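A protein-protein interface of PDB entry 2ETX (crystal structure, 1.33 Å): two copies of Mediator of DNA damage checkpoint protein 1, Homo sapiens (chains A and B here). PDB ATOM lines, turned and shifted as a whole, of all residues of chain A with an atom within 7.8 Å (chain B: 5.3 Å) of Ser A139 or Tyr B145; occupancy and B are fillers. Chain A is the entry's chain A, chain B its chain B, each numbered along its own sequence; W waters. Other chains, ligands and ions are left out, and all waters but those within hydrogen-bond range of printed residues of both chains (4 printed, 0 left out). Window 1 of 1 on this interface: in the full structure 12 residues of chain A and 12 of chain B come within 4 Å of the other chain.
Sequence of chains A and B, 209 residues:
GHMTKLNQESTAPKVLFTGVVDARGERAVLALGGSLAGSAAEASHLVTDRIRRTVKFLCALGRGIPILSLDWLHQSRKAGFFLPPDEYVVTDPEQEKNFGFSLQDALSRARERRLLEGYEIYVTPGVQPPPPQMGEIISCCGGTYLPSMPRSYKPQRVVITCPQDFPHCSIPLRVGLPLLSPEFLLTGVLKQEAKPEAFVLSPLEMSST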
ATOM      1  N   ALA A  41      17.381   5.165 -15.782  1.00  0.00           N
ATOM      2  CA  ALA A  41      16.648   6.139 -15.003  1.00  0.00           C
ATOM      3  C   ALA A  41      17.217   6.279 -13.583  1.00  0.00           C
ATOM      4  O   ALA A  41      17.081   7.322 -12.963  1.00  0.00           O
ATOM      5  CB  ALA A  41      15.157   5.792 -14.972  1.00  0.00           C
ATOM      6  N   CYS A  59      17.532   7.256 -22.487  1.00  0.00           N
ATOM      7  CA  CYS A  59      17.194   7.713 -21.135  1.00  0.00           C
ATOM      8  C   CYS A  59      18.365   8.434 -20.466  1.00  0.00           C
ATOM      9  O   CYS A  59      18.192   9.506 -19.870  1.00  0.00           O
ATOM     10  CB  CYS A  59      16.709   6.551 -20.282  1.00  0.00           C
ATOM     11  SG  CYS A  59      15.008   6.055 -20.652  1.00  0.00           S
ATOM     12  N   GLY A  62      18.744  11.781 -22.198  1.00  0.00           N
ATOM     13  CA  GLY A  62      17.662  12.692 -21.813  1.00  0.00           C
ATOM     14  C   GLY A  62      17.871  13.301 -20.433  1.00  0.00           C
ATOM     15  O   GLY A  62      17.540  14.461 -20.186  1.00  0.00           O
ATOM     16  N   ARG A  63      18.438  12.510 -19.522  1.00  0.00           N
ATOM     17  CA  ARG A  63      18.731  12.951 -18.160  1.00  0.00           C
ATOM     18  C   ARG A  63      20.013  13.772 -18.064  1.00  0.00           C
ATOM     19  O   ARG A  63      20.249  14.437 -17.040  1.00  0.00           O
ATOM     20  CB  ARG A  63      18.823  11.742 -17.224  1.00  0.00           C
ATOM     21  CG  ARG A  63      17.499  11.060 -16.989  1.00  0.00           C
ATOM     22  CD  ARG A  63      17.609   9.912 -16.002  1.00  0.00           C
ATOM     23  NE  ARG A  63      18.143  10.411 -14.732  1.00  0.00           N
ATOM     24  CZ  ARG A  63      19.136   9.856 -14.043  1.00  0.00           C
ATOM     25  NH1 ARG A  63      19.694   8.731 -14.461  1.00  0.00           N
ATOM     26  NH2 ARG A  63      19.545  10.432 -12.913  1.00  0.00           N
ATOM     27  N   ARG A 114      15.643  19.762 -19.555  1.00  0.00           N
ATOM     28  CA  ARG A 114      15.255  18.490 -20.150  1.00  0.00           C
ATOM     29  C   ARG A 114      14.296  18.731 -21.313  1.00  0.00           C
ATOM     30  O   ARG A 114      13.458  19.647 -21.300  1.00  0.00           O
ATOM     31  CB  ARG A 114      14.744  17.483 -19.123  1.00  0.00           C
ATOM     32  CG  ARG A 114      15.877  17.004 -18.203  1.00  0.00           C
ATOM     33  CD  ARG A 114      15.566  15.673 -17.564  1.00  0.00           C
ATOM     34  NE  ARG A 114      14.515  15.802 -16.565  1.00  0.00           N
ATOM     35  CZ  ARG A 114      13.980  14.780 -15.903  1.00  0.00           C
ATOM     36  NH1 ARG A 114      14.391  13.542 -16.152  1.00  0.00           N
ATOM     37  NH2 ARG A 114      13.041  14.996 -14.993  1.00  0.00           N
ATOM     38  N   LEU A 116      11.698  17.463 -22.822  1.00  0.00           N
ATOM     39  CA  LEU A 116      10.247  17.383 -22.869  1.00  0.00           C
ATOM     40  C   LEU A 116       9.573  18.030 -21.670  1.00  0.00           C
ATOM     41  O   LEU A 116       8.408  17.745 -21.367  1.00  0.00           O
ATOM     42  CB  LEU A 116       9.791  15.938 -23.059  1.00  0.00           C
ATOM     43  CG  LEU A 116      10.231  15.311 -24.382  1.00  0.00           C
ATOM     44  CD1 LEU A 116       9.880  13.827 -24.423  1.00  0.00           C
ATOM     45  CD2 LEU A 116       9.647  16.049 -25.589  1.00  0.00           C
ATOM     46  N   ILE A 121       2.312  13.450 -23.183  1.00  0.00           N
ATOM     47  CA  ILE A 121       2.335  12.590 -24.373  1.00  0.00           C
ATOM     48  C   ILE A 121       1.590  11.309 -24.092  1.00  0.00           C
ATOM     49  O   ILE A 121       1.925  10.589 -23.149  1.00  0.00           O
ATOM     50  CB  ILE A 121       3.780  12.273 -24.848  1.00  0.00           C
ATOM     51  CG1 ILE A 121       4.549  13.577 -25.072  1.00  0.00           C
ATOM     52  CG2 ILE A 121       3.750  11.392 -26.089  1.00  0.00           C
ATOM     53  CD1 ILE A 121       5.997  13.436 -25.565  1.00  0.00           C
ATOM     54  N   GLN A 133       8.073   1.443 -23.263  1.00  0.00           N
ATOM     55  CA  GLN A 133       9.434   1.898 -23.509  1.00  0.00           C
ATOM     56  C   GLN A 133       9.482   3.375 -23.883  1.00  0.00           C
ATOM     57  O   GLN A 133      10.336   4.120 -23.418  1.00  0.00           O
ATOM     58  CB  GLN A 133      10.067   1.087 -24.626  1.00  0.00           C
ATOM     59  CG  GLN A 133      10.278  -0.370 -24.241  1.00  0.00           C
ATOM     60  CD  GLN A 133      10.800  -1.198 -25.398  1.00  0.00           C
ATOM     61  OE1 GLN A 133      11.564  -0.700 -26.222  1.00  0.00           O
ATOM     62  NE2 GLN A 133      10.385  -2.470 -25.464  1.00  0.00           N
ATOM     63  N   MET A 134       8.555   3.790 -24.750  1.00  0.00           N
ATOM     64  CA  MET A 134       8.401   5.209 -25.088  1.00  0.00           C
ATOM     65  C   MET A 134       8.143   6.024 -23.813  1.00  0.00           C
ATOM     66  O   MET A 134       8.718   7.082 -23.627  1.00  0.00           O
ATOM     67  CB  MET A 134       7.274   5.407 -26.107  1.00  0.00           C
ATOM     68  CG  MET A 134       7.452   4.555 -27.365  1.00  0.00           C
ATOM     69  SD  MET A 134       8.829   5.113 -28.407  1.00  0.00           S
ATOM     70  CE  MET A 134       8.006   6.468 -29.243  1.00  0.00           C
ATOM     71  N   GLY A 135       7.288   5.518 -22.933  1.00  0.00           N
ATOM     72  CA  GLY A 135       7.000   6.175 -21.665  1.00  0.00           C
ATOM     73  C   GLY A 135       8.202   6.352 -20.765  1.00  0.00           C
ATOM     74  O   GLY A 135       8.358   7.402 -20.132  1.00  0.00           O
ATOM     75  N   GLU A 136       9.062   5.344 -20.699  1.00  0.00           N
ATOM     76  CA  GLU A 136      10.286   5.474 -19.929  1.00  0.00           C
ATOM     77  C   GLU A 136      11.134   6.623 -20.479  1.00  0.00           C
ATOM     78  O   GLU A 136      11.677   7.423 -19.719  1.00  0.00           O
ATOM     79  CB  GLU A 136      11.090   4.177 -19.992  1.00  0.00           C
ATOM     80  CG  GLU A 136      10.535   2.997 -19.217  1.00  0.00           C
ATOM     81  CD  GLU A 136      11.441   1.790 -19.334  1.00  0.00           C
ATOM     82  OE1 GLU A 136      11.215   0.934 -20.217  1.00  0.00           O
ATOM     83  OE2 GLU A 136      12.419   1.716 -18.566  1.00  0.00           O
ATOM     84  N   ILE A 137      11.280   6.693 -21.801  1.00  0.00           N
ATOM     85  CA  ILE A 137      12.081   7.737 -22.424  1.00  0.00           C
ATOM     86  C   ILE A 137      11.459   9.122 -22.180  1.00  0.00           C
ATOM     87  O   ILE A 137      12.164  10.079 -21.847  1.00  0.00           O
ATOM     88  CB  ILE A 137      12.288   7.453 -23.935  1.00  0.00           C
ATOM     89  CG1 ILE A 137      13.094   6.163 -24.111  1.00  0.00           C
ATOM     90  CG2 ILE A 137      12.992   8.623 -24.622  1.00  0.00           C
ATOM     91  CD1 ILE A 137      13.038   5.558 -25.516  1.00  0.00           C
ATOM     92  N   ILE A 138      10.141   9.216 -22.326  1.00  0.00           N
ATOM     93  CA  ILE A 138       9.431  10.477 -22.096  1.00  0.00           C
ATOM     94  C   ILE A 138       9.710  10.985 -20.676  1.00  0.00           C
ATOM     95  O   ILE A 138      10.039  12.159 -20.478  1.00  0.00           O
ATOM     96  CB  ILE A 138       7.917  10.309 -22.370  1.00  0.00           C
ATOM     97  CG1 ILE A 138       7.671  10.099 -23.870  1.00  0.00           C
ATOM     98  CG2 ILE A 138       7.124  11.498 -21.819  1.00  0.00           C
ATOM     99  CD1 ILE A 138       6.333   9.443 -24.176  1.00  0.00           C
ATOM    100  N   SER A 139       9.580  10.095 -19.693  1.00  0.00           N
ATOM    101  CA  SER A 139       9.805  10.462 -18.304  1.00  0.00           C
ATOM    102  C   SER A 139      11.260  10.903 -18.063  1.00  0.00           C
ATOM    103  O   SER A 139      11.519  11.909 -17.382  1.00  0.00           O
ATOM    104  CB  SER A 139       9.451   9.286 -17.417  1.00  0.00           C
ATOM    105  OG  SER A 139       9.648   9.650 -16.063  1.00  0.00           O
ATOM    106  N   CYS A 140      12.218  10.181 -18.649  1.00  0.00           N
ATOM    107  CA  CYS A 140      13.620  10.569 -18.474  1.00  0.00           C
ATOM    108  C   CYS A 140      13.969  11.905 -19.121  1.00  0.00           C
ATOM    109  O   CYS A 140      14.960  12.535 -18.761  1.00  0.00           O
ATOM    110  CB  CYS A 140      14.533   9.465 -18.982  1.00  0.00           C
ATOM    111  SG  CYS A 140      14.592   8.024 -17.836  1.00  0.00           S
ATOM    112  N   CYS A 141      13.137  12.344 -20.063  1.00  0.00           N
ATOM    113  CA  CYS A 141      13.300  13.665 -20.665  1.00  0.00           C
ATOM    114  C   CYS A 141      12.430  14.732 -20.016  1.00  0.00           C
ATOM    115  O   CYS A 141      12.277  15.820 -20.569  1.00  0.00           O
ATOM    116  CB  CYS A 141      13.025  13.616 -22.162  1.00  0.00           C
ATOM    117  SG  CYS A 141      14.167  12.604 -23.081  1.00  0.00           S
ATOM    118  N   GLY A 142      11.877  14.434 -18.845  1.00  0.00           N
ATOM    119  CA  GLY A 142      11.120  15.419 -18.074  1.00  0.00           C
ATOM    120  C   GLY A 142       9.699  15.668 -18.533  1.00  0.00           C
ATOM    121  O   GLY A 142       9.069  16.641 -18.078  1.00  0.00           O
ATOM    122  N   GLY A 143       9.187  14.811 -19.421  1.00  0.00           N
ATOM    123  CA  GLY A 143       7.802  14.899 -19.883  1.00  0.00           C
ATOM    124  C   GLY A 143       6.880  14.048 -19.046  1.00  0.00           C
ATOM    125  O   GLY A 143       7.313  13.302 -18.165  1.00  0.00           O
ATOM    126  N   THR A 144       5.584  14.214 -19.257  1.00  0.00           N
ATOM    127  CA  THR A 144       4.585  13.391 -18.601  1.00  0.00           C
ATOM    128  C   THR A 144       4.048  12.383 -19.595  1.00  0.00           C
ATOM    129  O   THR A 144       3.553  12.771 -20.658  1.00  0.00           O
ATOM    130  CB  THR A 144       3.410  14.249 -18.084  1.00  0.00           C
ATOM    131  OG1 THR A 144       3.901  15.232 -17.169  1.00  0.00           O
ATOM    132  CG2 THR A 144       2.371  13.375 -17.388  1.00  0.00           C
ATOM    133  N   TYR A 145       4.127  11.105 -19.257  1.00  0.00           N
ATOM    134  CA  TYR A 145       3.565  10.027 -20.044  1.00  0.00           C
ATOM    135  C   TYR A 145       2.136   9.816 -19.565  1.00  0.00           C
ATOM    136  O   TYR A 145       1.917   9.565 -18.385  1.00  0.00           O
ATOM    137  CB  TYR A 145       4.420   8.770 -19.826  1.00  0.00           C
ATOM    138  CG  TYR A 145       3.939   7.511 -20.504  1.00  0.00           C
ATOM    139  CD1 TYR A 145       3.807   7.451 -21.897  1.00  0.00           C
ATOM    140  CD2 TYR A 145       3.665   6.351 -19.767  1.00  0.00           C
ATOM    141  CE1 TYR A 145       3.407   6.289 -22.517  1.00  0.00           C
ATOM    142  CE2 TYR A 145       3.259   5.176 -20.390  1.00  0.00           C
ATOM    143  CZ  TYR A 145       3.128   5.165 -21.765  1.00  0.00           C
ATOM    144  OH  TYR A 145       2.705   4.014 -22.390  1.00  0.00           O
ATOM    145  N   LEU A 146       1.165   9.961 -20.460  1.00  0.00           N
ATOM    146  CA  LEU A 146      -0.246   9.865 -20.097  1.00  0.00           C
ATOM    147  C   LEU A 146      -0.768   8.444 -20.158  1.00  0.00           C
ATOM    148  O   LEU A 146      -0.423   7.700 -21.065  1.00  0.00           O
ATOM    149  CB  LEU A 146      -1.069  10.770 -21.007  1.00  0.00           C
ATOM    150  CG  LEU A 146      -0.743  12.266 -20.928  1.00  0.00           C
ATOM    151  CD1 LEU A 146      -1.537  12.992 -22.000  1.00  0.00           C
ATOM    152  CD2 LEU A 146      -1.070  12.845 -19.552  1.00  0.00           C
ATOM    153  N   PRO A 147      -1.617   8.051 -19.191  1.00  0.00           N
ATOM    154  CA  PRO A 147      -2.132   6.683 -19.177  1.00  0.00           C
ATOM    155  C   PRO A 147      -3.303   6.400 -20.118  1.00  0.00           C
ATOM    156  O   PRO A 147      -3.644   5.221 -20.320  1.00  0.00           O
ATOM    157  CB  PRO A 147      -2.584   6.504 -17.730  1.00  0.00           C
ATOM    158  CG  PRO A 147      -2.998   7.849 -17.322  1.00  0.00           C
ATOM    159  CD  PRO A 147      -2.034   8.806 -17.997  1.00  0.00           C
ATOM    160  N   LEU A 185       9.944  11.309 -30.948  1.00  0.00           N
ATOM    161  CA  LEU A 185      10.604  11.046 -29.686  1.00  0.00           C
ATOM    162  C   LEU A 185      12.015  10.511 -29.891  1.00  0.00           C
ATOM    163  O   LEU A 185      12.971  11.026 -29.308  1.00  0.00           O
ATOM    164  CB  LEU A 185       9.783  10.058 -28.848  1.00  0.00           C
ATOM    165  CG  LEU A 185      10.364   9.797 -27.445  1.00  0.00           C
ATOM    166  CD1 LEU A 185      10.284  11.072 -26.594  1.00  0.00           C
ATOM    167  CD2 LEU A 185       9.641   8.652 -26.769  1.00  0.00           C
ATOM    168  N   ILE B 121       0.782  11.329  -9.396  1.00  0.00           N
ATOM    169  CA  ILE B 121       1.689  11.003  -8.293  1.00  0.00           C
ATOM    170  C   ILE B 121       3.102  11.439  -8.617  1.00  0.00           C
ATOM    171  O   ILE B 121       3.651  11.018  -9.636  1.00  0.00           O
ATOM    172  CB  ILE B 121       1.655   9.489  -7.944  1.00  0.00           C
ATOM    173  CG1 ILE B 121       0.223   9.044  -7.651  1.00  0.00           C
ATOM    174  CG2 ILE B 121       2.618   9.179  -6.786  1.00  0.00           C
ATOM    175  CD1 ILE B 121       0.061   7.569  -7.320  1.00  0.00           C
ATOM    176  N   VAL B 123       6.986  11.250  -7.041  1.00  0.00           N
ATOM    177  CA  VAL B 123       7.766  10.455  -6.086  1.00  0.00           C
ATOM    178  C   VAL B 123       9.062  11.197  -5.887  1.00  0.00           C
ATOM    179  O   VAL B 123       9.822  11.379  -6.841  1.00  0.00           O
ATOM    180  CB  VAL B 123       8.013   9.020  -6.622  1.00  0.00           C
ATOM    181  CG1 VAL B 123       8.766   8.202  -5.573  1.00  0.00           C
ATOM    182  CG2 VAL B 123       6.706   8.333  -6.976  1.00  0.00           C
ATOM    183  N   PRO B 131      12.276   5.788  -7.342  1.00  0.00           N
ATOM    184  CA  PRO B 131      11.184   6.445  -8.082  1.00  0.00           C
ATOM    185  C   PRO B 131      10.849   5.851  -9.474  1.00  0.00           C
ATOM    186  O   PRO B 131       9.672   5.676  -9.754  1.00  0.00           O
ATOM    187  CB  PRO B 131      11.630   7.910  -8.166  1.00  0.00           C
ATOM    188  CG  PRO B 131      12.478   8.083  -6.912  1.00  0.00           C
ATOM    189  CD  PRO B 131      13.185   6.765  -6.706  1.00  0.00           C
ATOM    190  N   PRO B 132      11.846   5.536 -10.335  1.00  0.00           N
ATOM    191  CA  PRO B 132      11.443   5.023 -11.662  1.00  0.00           C
ATOM    192  C   PRO B 132      10.676   3.704 -11.591  1.00  0.00           C
ATOM    193  O   PRO B 132       9.763   3.499 -12.388  1.00  0.00           O
ATOM    194  CB  PRO B 132      12.775   4.856 -12.412  1.00  0.00           C
ATOM    195  CG  PRO B 132      13.782   5.653 -11.642  1.00  0.00           C
ATOM    196  CD  PRO B 132      13.311   5.690 -10.210  1.00  0.00           C
ATOM    197  N   MET B 134       8.699   2.830  -8.993  1.00  0.00           N
ATOM    198  CA  MET B 134       7.383   3.305  -8.532  1.00  0.00           C
ATOM    199  C   MET B 134       6.579   3.855  -9.719  1.00  0.00           C
ATOM    200  O   MET B 134       5.392   3.571  -9.858  1.00  0.00           O
ATOM    201  CB  MET B 134       7.546   4.353  -7.428  1.00  0.00           C
ATOM    202  CG  MET B 134       8.419   3.866  -6.251  1.00  0.00           C
ATOM    203  SD  MET B 134       7.612   2.565  -5.275  1.00  0.00           S
ATOM    204  CE  MET B 134       6.564   3.592  -4.238  1.00  0.00           C
ATOM    205  N   GLY B 135       7.236   4.619 -10.590  1.00  0.00           N
ATOM    206  CA  GLY B 135       6.568   5.154 -11.775  1.00  0.00           C
ATOM    207  C   GLY B 135       6.041   4.105 -12.732  1.00  0.00           C
ATOM    208  O   GLY B 135       4.947   4.249 -13.289  1.00  0.00           O
ATOM    209  N   ILE B 138       2.897   2.788 -11.046  1.00  0.00           N
ATOM    210  CA  ILE B 138       1.835   3.801 -11.146  1.00  0.00           C
ATOM    211  C   ILE B 138       1.181   3.765 -12.531  1.00  0.00           C
ATOM    212  O   ILE B 138      -0.050   3.758 -12.661  1.00  0.00           O
ATOM    213  CB  ILE B 138       2.395   5.205 -10.810  1.00  0.00           C
ATOM    214  CG1 ILE B 138       2.764   5.284  -9.321  1.00  0.00           C
ATOM    215  CG2 ILE B 138       1.408   6.298 -11.207  1.00  0.00           C
ATOM    216  CD1 ILE B 138       3.726   6.403  -8.957  1.00  0.00           C
ATOM    217  N   GLY B 143      -2.430   5.299 -13.471  1.00  0.00           N
ATOM    218  CA  GLY B 143      -2.149   6.622 -12.910  1.00  0.00           C
ATOM    219  C   GLY B 143      -1.158   7.388 -13.753  1.00  0.00           C
ATOM    220  O   GLY B 143      -0.591   6.858 -14.712  1.00  0.00           O
ATOM    221  N   THR B 144      -0.965   8.661 -13.434  1.00  0.00           N
ATOM    222  CA  THR B 144       0.036   9.483 -14.092  1.00  0.00           C
ATOM    223  C   THR B 144       1.210   9.685 -13.148  1.00  0.00           C
ATOM    224  O   THR B 144       1.009  10.153 -12.023  1.00  0.00           O
ATOM    225  CB  THR B 144      -0.538  10.872 -14.453  1.00  0.00           C
ATOM    226  OG1 THR B 144      -1.645  10.713 -15.348  1.00  0.00           O
ATOM    227  CG2 THR B 144       0.514  11.712 -15.137  1.00  0.00           C
ATOM    228  N   TYR B 145       2.416   9.335 -13.589  1.00  0.00           N
ATOM    229  CA  TYR B 145       3.652   9.564 -12.855  1.00  0.00           C
ATOM    230  C   TYR B 145       4.165  10.945 -13.257  1.00  0.00           C
ATOM    231  O   TYR B 145       4.383  11.197 -14.438  1.00  0.00           O
ATOM    232  CB  TYR B 145       4.654   8.465 -13.238  1.00  0.00           C
ATOM    233  CG  TYR B 145       6.022   8.562 -12.622  1.00  0.00           C
ATOM    234  CD1 TYR B 145       6.196   8.500 -11.237  1.00  0.00           C
ATOM    235  CD2 TYR B 145       7.157   8.647 -13.425  1.00  0.00           C
ATOM    236  CE1 TYR B 145       7.459   8.539 -10.684  1.00  0.00           C
ATOM    237  CE2 TYR B 145       8.422   8.703 -12.873  1.00  0.00           C
ATOM    238  CZ  TYR B 145       8.558   8.652 -11.506  1.00  0.00           C
ATOM    239  OH  TYR B 145       9.807   8.718 -10.949  1.00  0.00           O
ATOM    240  N   LEU B 146       4.316  11.853 -12.301  1.00  0.00           N
ATOM    241  CA  LEU B 146       4.709  13.236 -12.591  1.00  0.00           C
ATOM    242  C   LEU B 146       6.216  13.398 -12.636  1.00  0.00           C
ATOM    243  O   LEU B 146       6.919  12.783 -11.859  1.00  0.00           O
ATOM    244  CB  LEU B 146       4.104  14.179 -11.555  1.00  0.00           C
ATOM    245  CG  LEU B 146       2.575  14.232 -11.492  1.00  0.00           C
ATOM    246  CD1 LEU B 146       2.133  15.093 -10.331  1.00  0.00           C
ATOM    247  CD2 LEU B 146       1.973  14.758 -12.804  1.00  0.00           C
ATOM    248  N   PRO B 147       6.719  14.226 -13.563  1.00  0.00           N
ATOM    249  CA  PRO B 147       8.160  14.385 -13.692  1.00  0.00           C
ATOM    250  C   PRO B 147       8.805  15.343 -12.699  1.00  0.00           C
ATOM    251  O   PRO B 147      10.034  15.323 -12.548  1.00  0.00           O
ATOM    252  CB  PRO B 147       8.318  14.912 -15.119  1.00  0.00           C
ATOM    253  CG  PRO B 147       7.097  15.664 -15.349  1.00  0.00           C
ATOM    254  CD  PRO B 147       5.991  14.926 -14.635  1.00  0.00           C
HETATM  255  O   HOH W   1       7.530  11.742 -15.786  1.00  0.00           O
HETATM  256  O   HOH W   2       2.819   8.162 -16.185  1.00  0.00           O
HETATM  257  O   HOH W   3       5.382  10.231 -16.787  1.00  0.00           O
HETATM  258  O   HOH W   4      12.052  17.314 -14.055  1.00  0.00           O
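The backbone carbonyl oxygen (O) of Thr A144 lies within hydrogen-bond range of the backbone NH (N) of Ile A121 (2.9 Å).
O of Ile B138 sits at hydrogen-bond distance from N of Gly B143 (2.9 Å).
The backbone carbonyl oxygen (O) of Thr B144 lies within hydrogen-bond range of the backbone NH (N) of Ile B121, at 2.9 Å.
The backbone carbonyl oxygen (O) of Ile A138 is in hydrogen-bond range of the backbone NH (N) of Gly A143, 3.0 Å away.
The backbone carbonyl oxygen (O) of Ala A41 is in hydrogen-bond range of the guanidinium group (NH1) of Arg A63, at 3.3 Å.
The side-chain hydroxyl (OH) of Tyr B145 sits at hydrogen-bond distance from the backbone carbonyl oxygen (O) of Pro B131, 3.3 Å away.
Gly A143 touches Pro B147, and with the chains exchanged Pro A147 touches Gly B143.
Thr B144 touches its own counterpart, Thr A144.
Thr A144 touches Pro B147, and with the chains exchanged Pro A147 touches Thr B144.
9 positions are printed for both chains.
Of the printed residues of chain B, Ala A41 touches Pro B132 (3.6 Å).
Of the printed residues of chain B, Gly A143 touches Pro B147 (3.6 Å).
Leu A146 touches none of the printed residues of chain B.
Of the printed residues of chain B, Pro A147 touches Gly B143 (3.6 Å) and Thr B144 (3.3 Å).
Printed residues of chain A within 4 Å of Gly B143: Pro A147 (3.6 Å).
Tyr B145 touches just one residue of chain A: Ser A139 (3.5 Å).
Of the printed residues of chain A, Pro B147 touches Arg A114, Gly A142, Gly A143 and Thr A144.
The nearest printed residue of chain A that does not touch Thr B144 is Tyr A145 (4.1 Å).
Among the printed residues, merely in contact across the chains: Pro A147 with Thr B144, Thr A144 with Pro B147, Thr A144 with Thr B144, Gly A142 with Pro B147, Ser A139 with Tyr B145, Gly A143 with Pro B147, Ala A41 with Pro B132, Pro A147 with Gly B143 and Arg A114 with Pro B147.
Water W4 lies within hydrogen-bond range of the guanidinium group (NH2) of Arg A114 (2.7 Å) and the backbone carbonyl oxygen (O) of Pro B147 (3.2 Å).
Water W3 lies within hydrogen-bond range of O of Tyr B145 and N of Tyr A145.
Water W2 bridges the backbone carbonyl oxygen (O) of Tyr A145 (2.8 Å) and the backbone NH (N) of Tyr B145 (2.9 Å).
Water W1 lies within hydrogen-bond range of O of Gly A143 (2.9 Å), OG of Ser A139 (3.0 Å) and O of Tyr B145 (3.5 Å).
Among the printed residues, no Asp or Glu carboxylate lies within 4 Å of a Lys or Arg side-chain nitrogen of the other chain.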
